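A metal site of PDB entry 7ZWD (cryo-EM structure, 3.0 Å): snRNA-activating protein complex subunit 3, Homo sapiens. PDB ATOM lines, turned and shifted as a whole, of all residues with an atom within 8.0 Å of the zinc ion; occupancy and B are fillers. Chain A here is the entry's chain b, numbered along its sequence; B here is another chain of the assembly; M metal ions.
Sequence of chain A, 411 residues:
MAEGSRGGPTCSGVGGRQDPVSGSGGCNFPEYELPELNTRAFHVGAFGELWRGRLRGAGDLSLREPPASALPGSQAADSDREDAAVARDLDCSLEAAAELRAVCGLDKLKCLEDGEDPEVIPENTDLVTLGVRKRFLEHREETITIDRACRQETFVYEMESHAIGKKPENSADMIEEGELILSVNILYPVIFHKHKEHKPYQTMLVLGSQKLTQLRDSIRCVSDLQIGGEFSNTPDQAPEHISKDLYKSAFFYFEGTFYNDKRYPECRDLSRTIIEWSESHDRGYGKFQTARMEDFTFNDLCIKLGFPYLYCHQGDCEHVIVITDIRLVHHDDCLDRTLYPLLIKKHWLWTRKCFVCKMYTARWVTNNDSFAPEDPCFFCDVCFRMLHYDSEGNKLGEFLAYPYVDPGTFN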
ATOM      1  N   LYS A 353     -15.608  12.537   9.434  1.00  0.00           N
ATOM      2  CA  LYS A 353     -16.966  12.161   9.102  1.00  0.00           C
ATOM      3  C   LYS A 353     -16.982  10.942   8.206  1.00  0.00           C
ATOM      4  O   LYS A 353     -15.971  10.564   7.618  1.00  0.00           O
ATOM      5  CB  LYS A 353     -17.703  13.325   8.419  1.00  0.00           C
ATOM      6  CG  LYS A 353     -17.989  14.483   9.328  1.00  0.00           C
ATOM      7  CD  LYS A 353     -19.276  15.134   8.924  1.00  0.00           C
ATOM      8  CE  LYS A 353     -19.283  16.597   9.283  1.00  0.00           C
ATOM      9  NZ  LYS A 353     -18.196  17.303   8.572  1.00  0.00           N
ATOM     10  N   CYS A 354     -18.154  10.325   8.115  1.00  0.00           N
ATOM     11  CA  CYS A 354     -18.349   9.231   7.175  1.00  0.00           C
ATOM     12  C   CYS A 354     -18.001   9.699   5.776  1.00  0.00           C
ATOM     13  O   CYS A 354     -18.376  10.785   5.347  1.00  0.00           O
ATOM     14  CB  CYS A 354     -19.798   8.750   7.224  1.00  0.00           C
ATOM     15  SG  CYS A 354     -20.249   7.668   5.878  1.00  0.00           S
ATOM     16  N   PHE A 355     -17.259   8.868   5.062  1.00  0.00           N
ATOM     17  CA  PHE A 355     -16.797   9.260   3.740  1.00  0.00           C
ATOM     18  C   PHE A 355     -17.887   9.146   2.690  1.00  0.00           C
ATOM     19  O   PHE A 355     -17.801   9.840   1.669  1.00  0.00           O
ATOM     20  CB  PHE A 355     -15.602   8.428   3.317  1.00  0.00           C
ATOM     21  CG  PHE A 355     -14.299   8.978   3.787  1.00  0.00           C
ATOM     22  CD1 PHE A 355     -14.258   9.927   4.784  1.00  0.00           C
ATOM     23  CD2 PHE A 355     -13.119   8.563   3.229  1.00  0.00           C
ATOM     24  CE1 PHE A 355     -13.059  10.432   5.224  1.00  0.00           C
ATOM     25  CE2 PHE A 355     -11.920   9.069   3.669  1.00  0.00           C
ATOM     26  CZ  PHE A 355     -11.888  10.006   4.663  1.00  0.00           C
ATOM     27  N   VAL A 356     -18.892   8.316   2.906  1.00  0.00           N
ATOM     28  CA  VAL A 356     -19.976   8.165   1.953  1.00  0.00           C
ATOM     29  C   VAL A 356     -20.955   9.316   2.057  1.00  0.00           C
ATOM     30  O   VAL A 356     -21.093  10.116   1.135  1.00  0.00           O
ATOM     31  CB  VAL A 356     -20.688   6.815   2.169  1.00  0.00           C
ATOM     32  CG1 VAL A 356     -21.811   6.693   1.200  1.00  0.00           C
ATOM     33  CG2 VAL A 356     -19.726   5.687   1.994  1.00  0.00           C
ATOM     34  N   CYS A 357     -21.628   9.443   3.195  1.00  0.00           N
ATOM     35  CA  CYS A 357     -22.427  10.618   3.498  1.00  0.00           C
ATOM     36  C   CYS A 357     -21.692  11.408   4.563  1.00  0.00           C
ATOM     37  O   CYS A 357     -21.198  10.853   5.546  1.00  0.00           O
ATOM     38  CB  CYS A 357     -23.819  10.248   4.006  1.00  0.00           C
ATOM     39  SG  CYS A 357     -23.837   9.444   5.610  1.00  0.00           S
ATOM     40  N   LYS A 358     -21.619  12.707   4.366  1.00  0.00           N
ATOM     41  CA  LYS A 358     -20.876  13.567   5.282  1.00  0.00           C
ATOM     42  C   LYS A 358     -21.769  14.109   6.383  1.00  0.00           C
ATOM     43  O   LYS A 358     -21.555  15.234   6.842  1.00  0.00           O
ATOM     44  CB  LYS A 358     -20.220  14.700   4.512  1.00  0.00           C
ATOM     45  CG  LYS A 358     -19.475  14.255   3.297  1.00  0.00           C
ATOM     46  CD  LYS A 358     -18.155  13.631   3.670  1.00  0.00           C
ATOM     47  CE  LYS A 358     -17.492  13.036   2.446  1.00  0.00           C
ATOM     48  NZ  LYS A 358     -17.434  13.995   1.318  1.00  0.00           N
ATOM     49  N   MET A 359     -22.772  13.348   6.805  1.00  0.00           N
ATOM     50  CA  MET A 359     -23.686  13.820   7.833  1.00  0.00           C
ATOM     51  C   MET A 359     -23.350  13.292   9.215  1.00  0.00           C
ATOM     52  O   MET A 359     -23.671  13.956  10.204  1.00  0.00           O
ATOM     53  CB  MET A 359     -25.123  13.433   7.478  1.00  0.00           C
ATOM     54  CG  MET A 359     -25.569  13.929   6.124  1.00  0.00           C
ATOM     55  SD  MET A 359     -25.116  15.656   5.885  1.00  0.00           S
ATOM     56  CE  MET A 359     -25.599  15.905   4.177  1.00  0.00           C
ATOM     57  N   TYR A 360     -22.727  12.121   9.321  1.00  0.00           N
ATOM     58  CA  TYR A 360     -22.430  11.532  10.607  1.00  0.00           C
ATOM     59  C   TYR A 360     -20.935  11.346  10.753  1.00  0.00           C
ATOM     60  O   TYR A 360     -20.186  11.389   9.789  1.00  0.00           O
ATOM     61  CB  TYR A 360     -23.134  10.191  10.788  1.00  0.00           C
ATOM     62  CG  TYR A 360     -24.610  10.258  10.548  1.00  0.00           C
ATOM     63  CD1 TYR A 360     -25.444  10.936  11.411  1.00  0.00           C
ATOM     64  CD2 TYR A 360     -25.177   9.634   9.459  1.00  0.00           C
ATOM     65  CE1 TYR A 360     -26.787  11.002  11.191  1.00  0.00           C
ATOM     66  CE2 TYR A 360     -26.529   9.688   9.238  1.00  0.00           C
ATOM     67  CZ  TYR A 360     -27.321  10.372  10.106  1.00  0.00           C
ATOM     68  OH  TYR A 360     -28.678  10.437   9.892  1.00  0.00           O
ATOM     69  N   THR A 361     -20.508  11.145  11.989  1.00  0.00           N
ATOM     70  CA  THR A 361     -19.087  10.966  12.249  1.00  0.00           C
ATOM     71  C   THR A 361     -18.683   9.532  11.971  1.00  0.00           C
ATOM     72  O   THR A 361     -19.521   8.640  11.857  1.00  0.00           O
ATOM     73  CB  THR A 361     -18.744  11.315  13.681  1.00  0.00           C
ATOM     74  OG1 THR A 361     -17.322  11.355  13.826  1.00  0.00           O
ATOM     75  CG2 THR A 361     -19.285  10.268  14.600  1.00  0.00           C
ATOM     76  N   ALA A 362     -17.389   9.325  11.887  1.00  0.00           N
ATOM     77  CA  ALA A 362     -16.856   8.017  11.563  1.00  0.00           C
ATOM     78  C   ALA A 362     -16.832   7.109  12.777  1.00  0.00           C
ATOM     79  O   ALA A 362     -16.175   7.406  13.775  1.00  0.00           O
ATOM     80  CB  ALA A 362     -15.449   8.165  11.016  1.00  0.00           C
ATOM     81  N   PHE A 378     -13.227   5.947   6.296  1.00  0.00           N
ATOM     82  CA  PHE A 378     -13.989   6.077   7.531  1.00  0.00           C
ATOM     83  C   PHE A 378     -15.474   6.093   7.214  1.00  0.00           C
ATOM     84  O   PHE A 378     -15.912   6.765   6.284  1.00  0.00           O
ATOM     85  CB  PHE A 378     -13.602   7.359   8.260  1.00  0.00           C
ATOM     86  CG  PHE A 378     -12.141   7.495   8.503  1.00  0.00           C
ATOM     87  CD1 PHE A 378     -11.581   6.990   9.639  1.00  0.00           C
ATOM     88  CD2 PHE A 378     -11.345   8.124   7.596  1.00  0.00           C
ATOM     89  CE1 PHE A 378     -10.245   7.121   9.861  1.00  0.00           C
ATOM     90  CE2 PHE A 378     -10.009   8.255   7.818  1.00  0.00           C
ATOM     91  CZ  PHE A 378      -9.466   7.745   8.952  1.00  0.00           C
ATOM     92  N   PHE A 379     -16.245   5.369   8.007  1.00  0.00           N
ATOM     93  CA  PHE A 379     -17.677   5.260   7.799  1.00  0.00           C
ATOM     94  C   PHE A 379     -18.413   5.482   9.102  1.00  0.00           C
ATOM     95  O   PHE A 379     -17.882   5.243  10.181  1.00  0.00           O
ATOM     96  CB  PHE A 379     -18.066   3.885   7.269  1.00  0.00           C
ATOM     97  CG  PHE A 379     -17.396   3.521   5.995  1.00  0.00           C
ATOM     98  CD1 PHE A 379     -17.973   3.806   4.780  1.00  0.00           C
ATOM     99  CD2 PHE A 379     -16.188   2.853   6.003  1.00  0.00           C
ATOM    100  CE1 PHE A 379     -17.372   3.455   3.614  1.00  0.00           C
ATOM    101  CE2 PHE A 379     -15.583   2.508   4.831  1.00  0.00           C
ATOM    102  CZ  PHE A 379     -16.174   2.809   3.637  1.00  0.00           C
ATOM    103  N   CYS A 380     -19.646   5.968   8.983  1.00  0.00           N
ATOM    104  CA  CYS A 380     -20.579   5.900  10.089  1.00  0.00           C
ATOM    105  C   CYS A 380     -21.095   4.474  10.198  1.00  0.00           C
ATOM    106  O   CYS A 380     -20.693   3.592   9.441  1.00  0.00           O
ATOM    107  CB  CYS A 380     -21.716   6.897   9.905  1.00  0.00           C
ATOM    108  SG  CYS A 380     -22.519   6.822   8.297  1.00  0.00           S
ATOM    109  N   ASP A 381     -21.991   4.240  11.143  1.00  0.00           N
ATOM    110  CA  ASP A 381     -22.517   2.888  11.272  1.00  0.00           C
ATOM    111  C   ASP A 381     -23.440   2.553  10.106  1.00  0.00           C
ATOM    112  O   ASP A 381     -23.405   1.429   9.580  1.00  0.00           O
ATOM    113  CB  ASP A 381     -23.261   2.738  12.591  1.00  0.00           C
ATOM    114  CG  ASP A 381     -23.239   1.317  13.116  1.00  0.00           C
ATOM    115  OD1 ASP A 381     -22.133   0.797  13.347  1.00  0.00           O
ATOM    116  OD2 ASP A 381     -24.327   0.730  13.273  1.00  0.00           O
ATOM    117  N   VAL A 382     -24.250   3.509   9.675  1.00  0.00           N
ATOM    118  CA  VAL A 382     -25.207   3.253   8.598  1.00  0.00           C
ATOM    119  C   VAL A 382     -24.490   2.902   7.309  1.00  0.00           C
ATOM    120  O   VAL A 382     -24.712   1.828   6.731  1.00  0.00           O
ATOM    121  CB  VAL A 382     -26.124   4.471   8.407  1.00  0.00           C
ATOM    122  CG1 VAL A 382     -27.182   4.163   7.393  1.00  0.00           C
ATOM    123  CG2 VAL A 382     -26.741   4.879   9.719  1.00  0.00           C
ATOM    124  N   CYS A 383     -23.618   3.787   6.848  1.00  0.00           N
ATOM    125  CA  CYS A 383     -22.924   3.543   5.588  1.00  0.00           C
ATOM    126  C   CYS A 383     -21.960   2.382   5.660  1.00  0.00           C
ATOM    127  O   CYS A 383     -21.547   1.861   4.630  1.00  0.00           O
ATOM    128  CB  CYS A 383     -22.189   4.809   5.153  1.00  0.00           C
ATOM    129  SG  CYS A 383     -23.256   6.230   4.957  1.00  0.00           S
ATOM    130  N   PHE A 384     -21.571   1.970   6.858  1.00  0.00           N
ATOM    131  CA  PHE A 384     -20.748   0.769   6.976  1.00  0.00           C
ATOM    132  C   PHE A 384     -21.594  -0.483   6.807  1.00  0.00           C
ATOM    133  O   PHE A 384     -21.267  -1.368   6.020  1.00  0.00           O
ATOM    134  CB  PHE A 384     -20.053   0.762   8.329  1.00  0.00           C
ATOM    135  CG  PHE A 384     -19.166  -0.413   8.542  1.00  0.00           C
ATOM    136  CD1 PHE A 384     -17.924  -0.464   7.951  1.00  0.00           C
ATOM    137  CD2 PHE A 384     -19.574  -1.454   9.339  1.00  0.00           C
ATOM    138  CE1 PHE A 384     -17.106  -1.546   8.158  1.00  0.00           C
ATOM    139  CE2 PHE A 384     -18.756  -2.535   9.546  1.00  0.00           C
ATOM    140  CZ  PHE A 384     -17.522  -2.581   8.955  1.00  0.00           C
ATOM    141  N   MET A 386     -24.341  -0.763   5.311  1.00  0.00           N
ATOM    142  CA  MET A 386     -24.993  -0.795   4.016  1.00  0.00           C
ATOM    143  C   MET A 386     -24.051  -1.165   2.886  1.00  0.00           C
ATOM    144  O   MET A 386     -24.523  -1.619   1.837  1.00  0.00           O
ATOM    145  CB  MET A 386     -25.622   0.563   3.705  1.00  0.00           C
ATOM    146  CG  MET A 386     -26.857   0.862   4.511  1.00  0.00           C
ATOM    147  SD  MET A 386     -27.571   2.437   4.046  1.00  0.00           S
ATOM    148  CE  MET A 386     -27.727   2.192   2.294  1.00  0.00           C
ATOM    149  N   LEU B 334     -23.613   4.195  -3.698  1.00  0.00           N
ATOM    150  CA  LEU B 334     -24.045   4.400  -2.320  1.00  0.00           C
ATOM    151  C   LEU B 334     -23.972   5.873  -1.937  1.00  0.00           C
ATOM    152  O   LEU B 334     -24.854   6.387  -1.237  1.00  0.00           O
ATOM    153  CB  LEU B 334     -23.191   3.572  -1.373  1.00  0.00           C
ATOM    154  CG  LEU B 334     -23.478   3.780   0.107  1.00  0.00           C
ATOM    155  CD1 LEU B 334     -24.849   3.254   0.417  1.00  0.00           C
ATOM    156  CD2 LEU B 334     -22.445   3.074   0.927  1.00  0.00           C
ATOM    157  N   GLN B 338     -27.186   8.048  -0.678  1.00  0.00           N
ATOM    158  CA  GLN B 338     -27.251   8.745   0.598  1.00  0.00           C
ATOM    159  C   GLN B 338     -27.492  10.240   0.392  1.00  0.00           C
ATOM    160  O   GLN B 338     -28.443  10.802   0.938  1.00  0.00           O
ATOM    161  CB  GLN B 338     -26.008   8.491   1.432  1.00  0.00           C
ATOM    162  CG  GLN B 338     -25.791   7.038   1.747  1.00  0.00           C
ATOM    163  CD  GLN B 338     -26.732   6.523   2.791  1.00  0.00           C
ATOM    164  OE1 GLN B 338     -27.851   6.122   2.490  1.00  0.00           O
ATOM    165  NE2 GLN B 338     -26.276   6.501   4.038  1.00  0.00           N
ATOM    166  N   GLN B 339     -26.657  10.879  -0.424  1.00  0.00           N
ATOM    167  CA  GLN B 339     -26.818  12.313  -0.649  1.00  0.00           C
ATOM    168  C   GLN B 339     -28.172  12.650  -1.251  1.00  0.00           C
ATOM    169  O   GLN B 339     -28.529  13.837  -1.312  1.00  0.00           O
ATOM    170  CB  GLN B 339     -25.702  12.840  -1.558  1.00  0.00           C
ATOM    171  CG  GLN B 339     -24.309  12.729  -0.966  1.00  0.00           C
ATOM    172  CD  GLN B 339     -24.222  13.287   0.450  1.00  0.00           C
ATOM    173  OE1 GLN B 339     -24.324  12.550   1.430  1.00  0.00           O
ATOM    174  NE2 GLN B 339     -24.014  14.589   0.561  1.00  0.00           N
ATOM    175  N   LEU B 344     -32.199   9.224   5.958  1.00  0.00           N
ATOM    176  CA  LEU B 344     -30.877   9.309   6.566  1.00  0.00           C
ATOM    177  C   LEU B 344     -30.949   9.934   7.943  1.00  0.00           C
ATOM    178  O   LEU B 344     -30.416   9.398   8.910  1.00  0.00           O
ATOM    179  CB  LEU B 344     -29.952  10.102   5.653  1.00  0.00           C
ATOM    180  CG  LEU B 344     -28.477  10.076   6.018  1.00  0.00           C
ATOM    181  CD1 LEU B 344     -27.953   8.666   5.928  1.00  0.00           C
ATOM    182  CD2 LEU B 344     -27.704  11.001   5.107  1.00  0.00           C
HETATM  183 ZN    ZN M   1     -22.305   7.652   6.281  1.00  0.00          ZN
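The nearest printed residue that does not touch the zinc ion is Val 356 (4.5 Å).
SG of Cys 383 sits close to NE2 of Gln 338 of chain B. The backbone NH (N) of Cys 354 lies within hydrogen-bond range of the backbone carbonyl oxygen (O) of Tyr 360, at 2.8 Å. SG of Cys 354 lies close to N of Val 356, 3.3 Å away.
The zinc ion is bound by the side-chain sulfur of Cys 354 (2.1 Å), the side-chain sulfur of Cys 383 (2.2 Å), the side-chain sulfur of Cys 380 (2.2 Å) and the side-chain sulfur of Cys 357 (2.5 Å).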
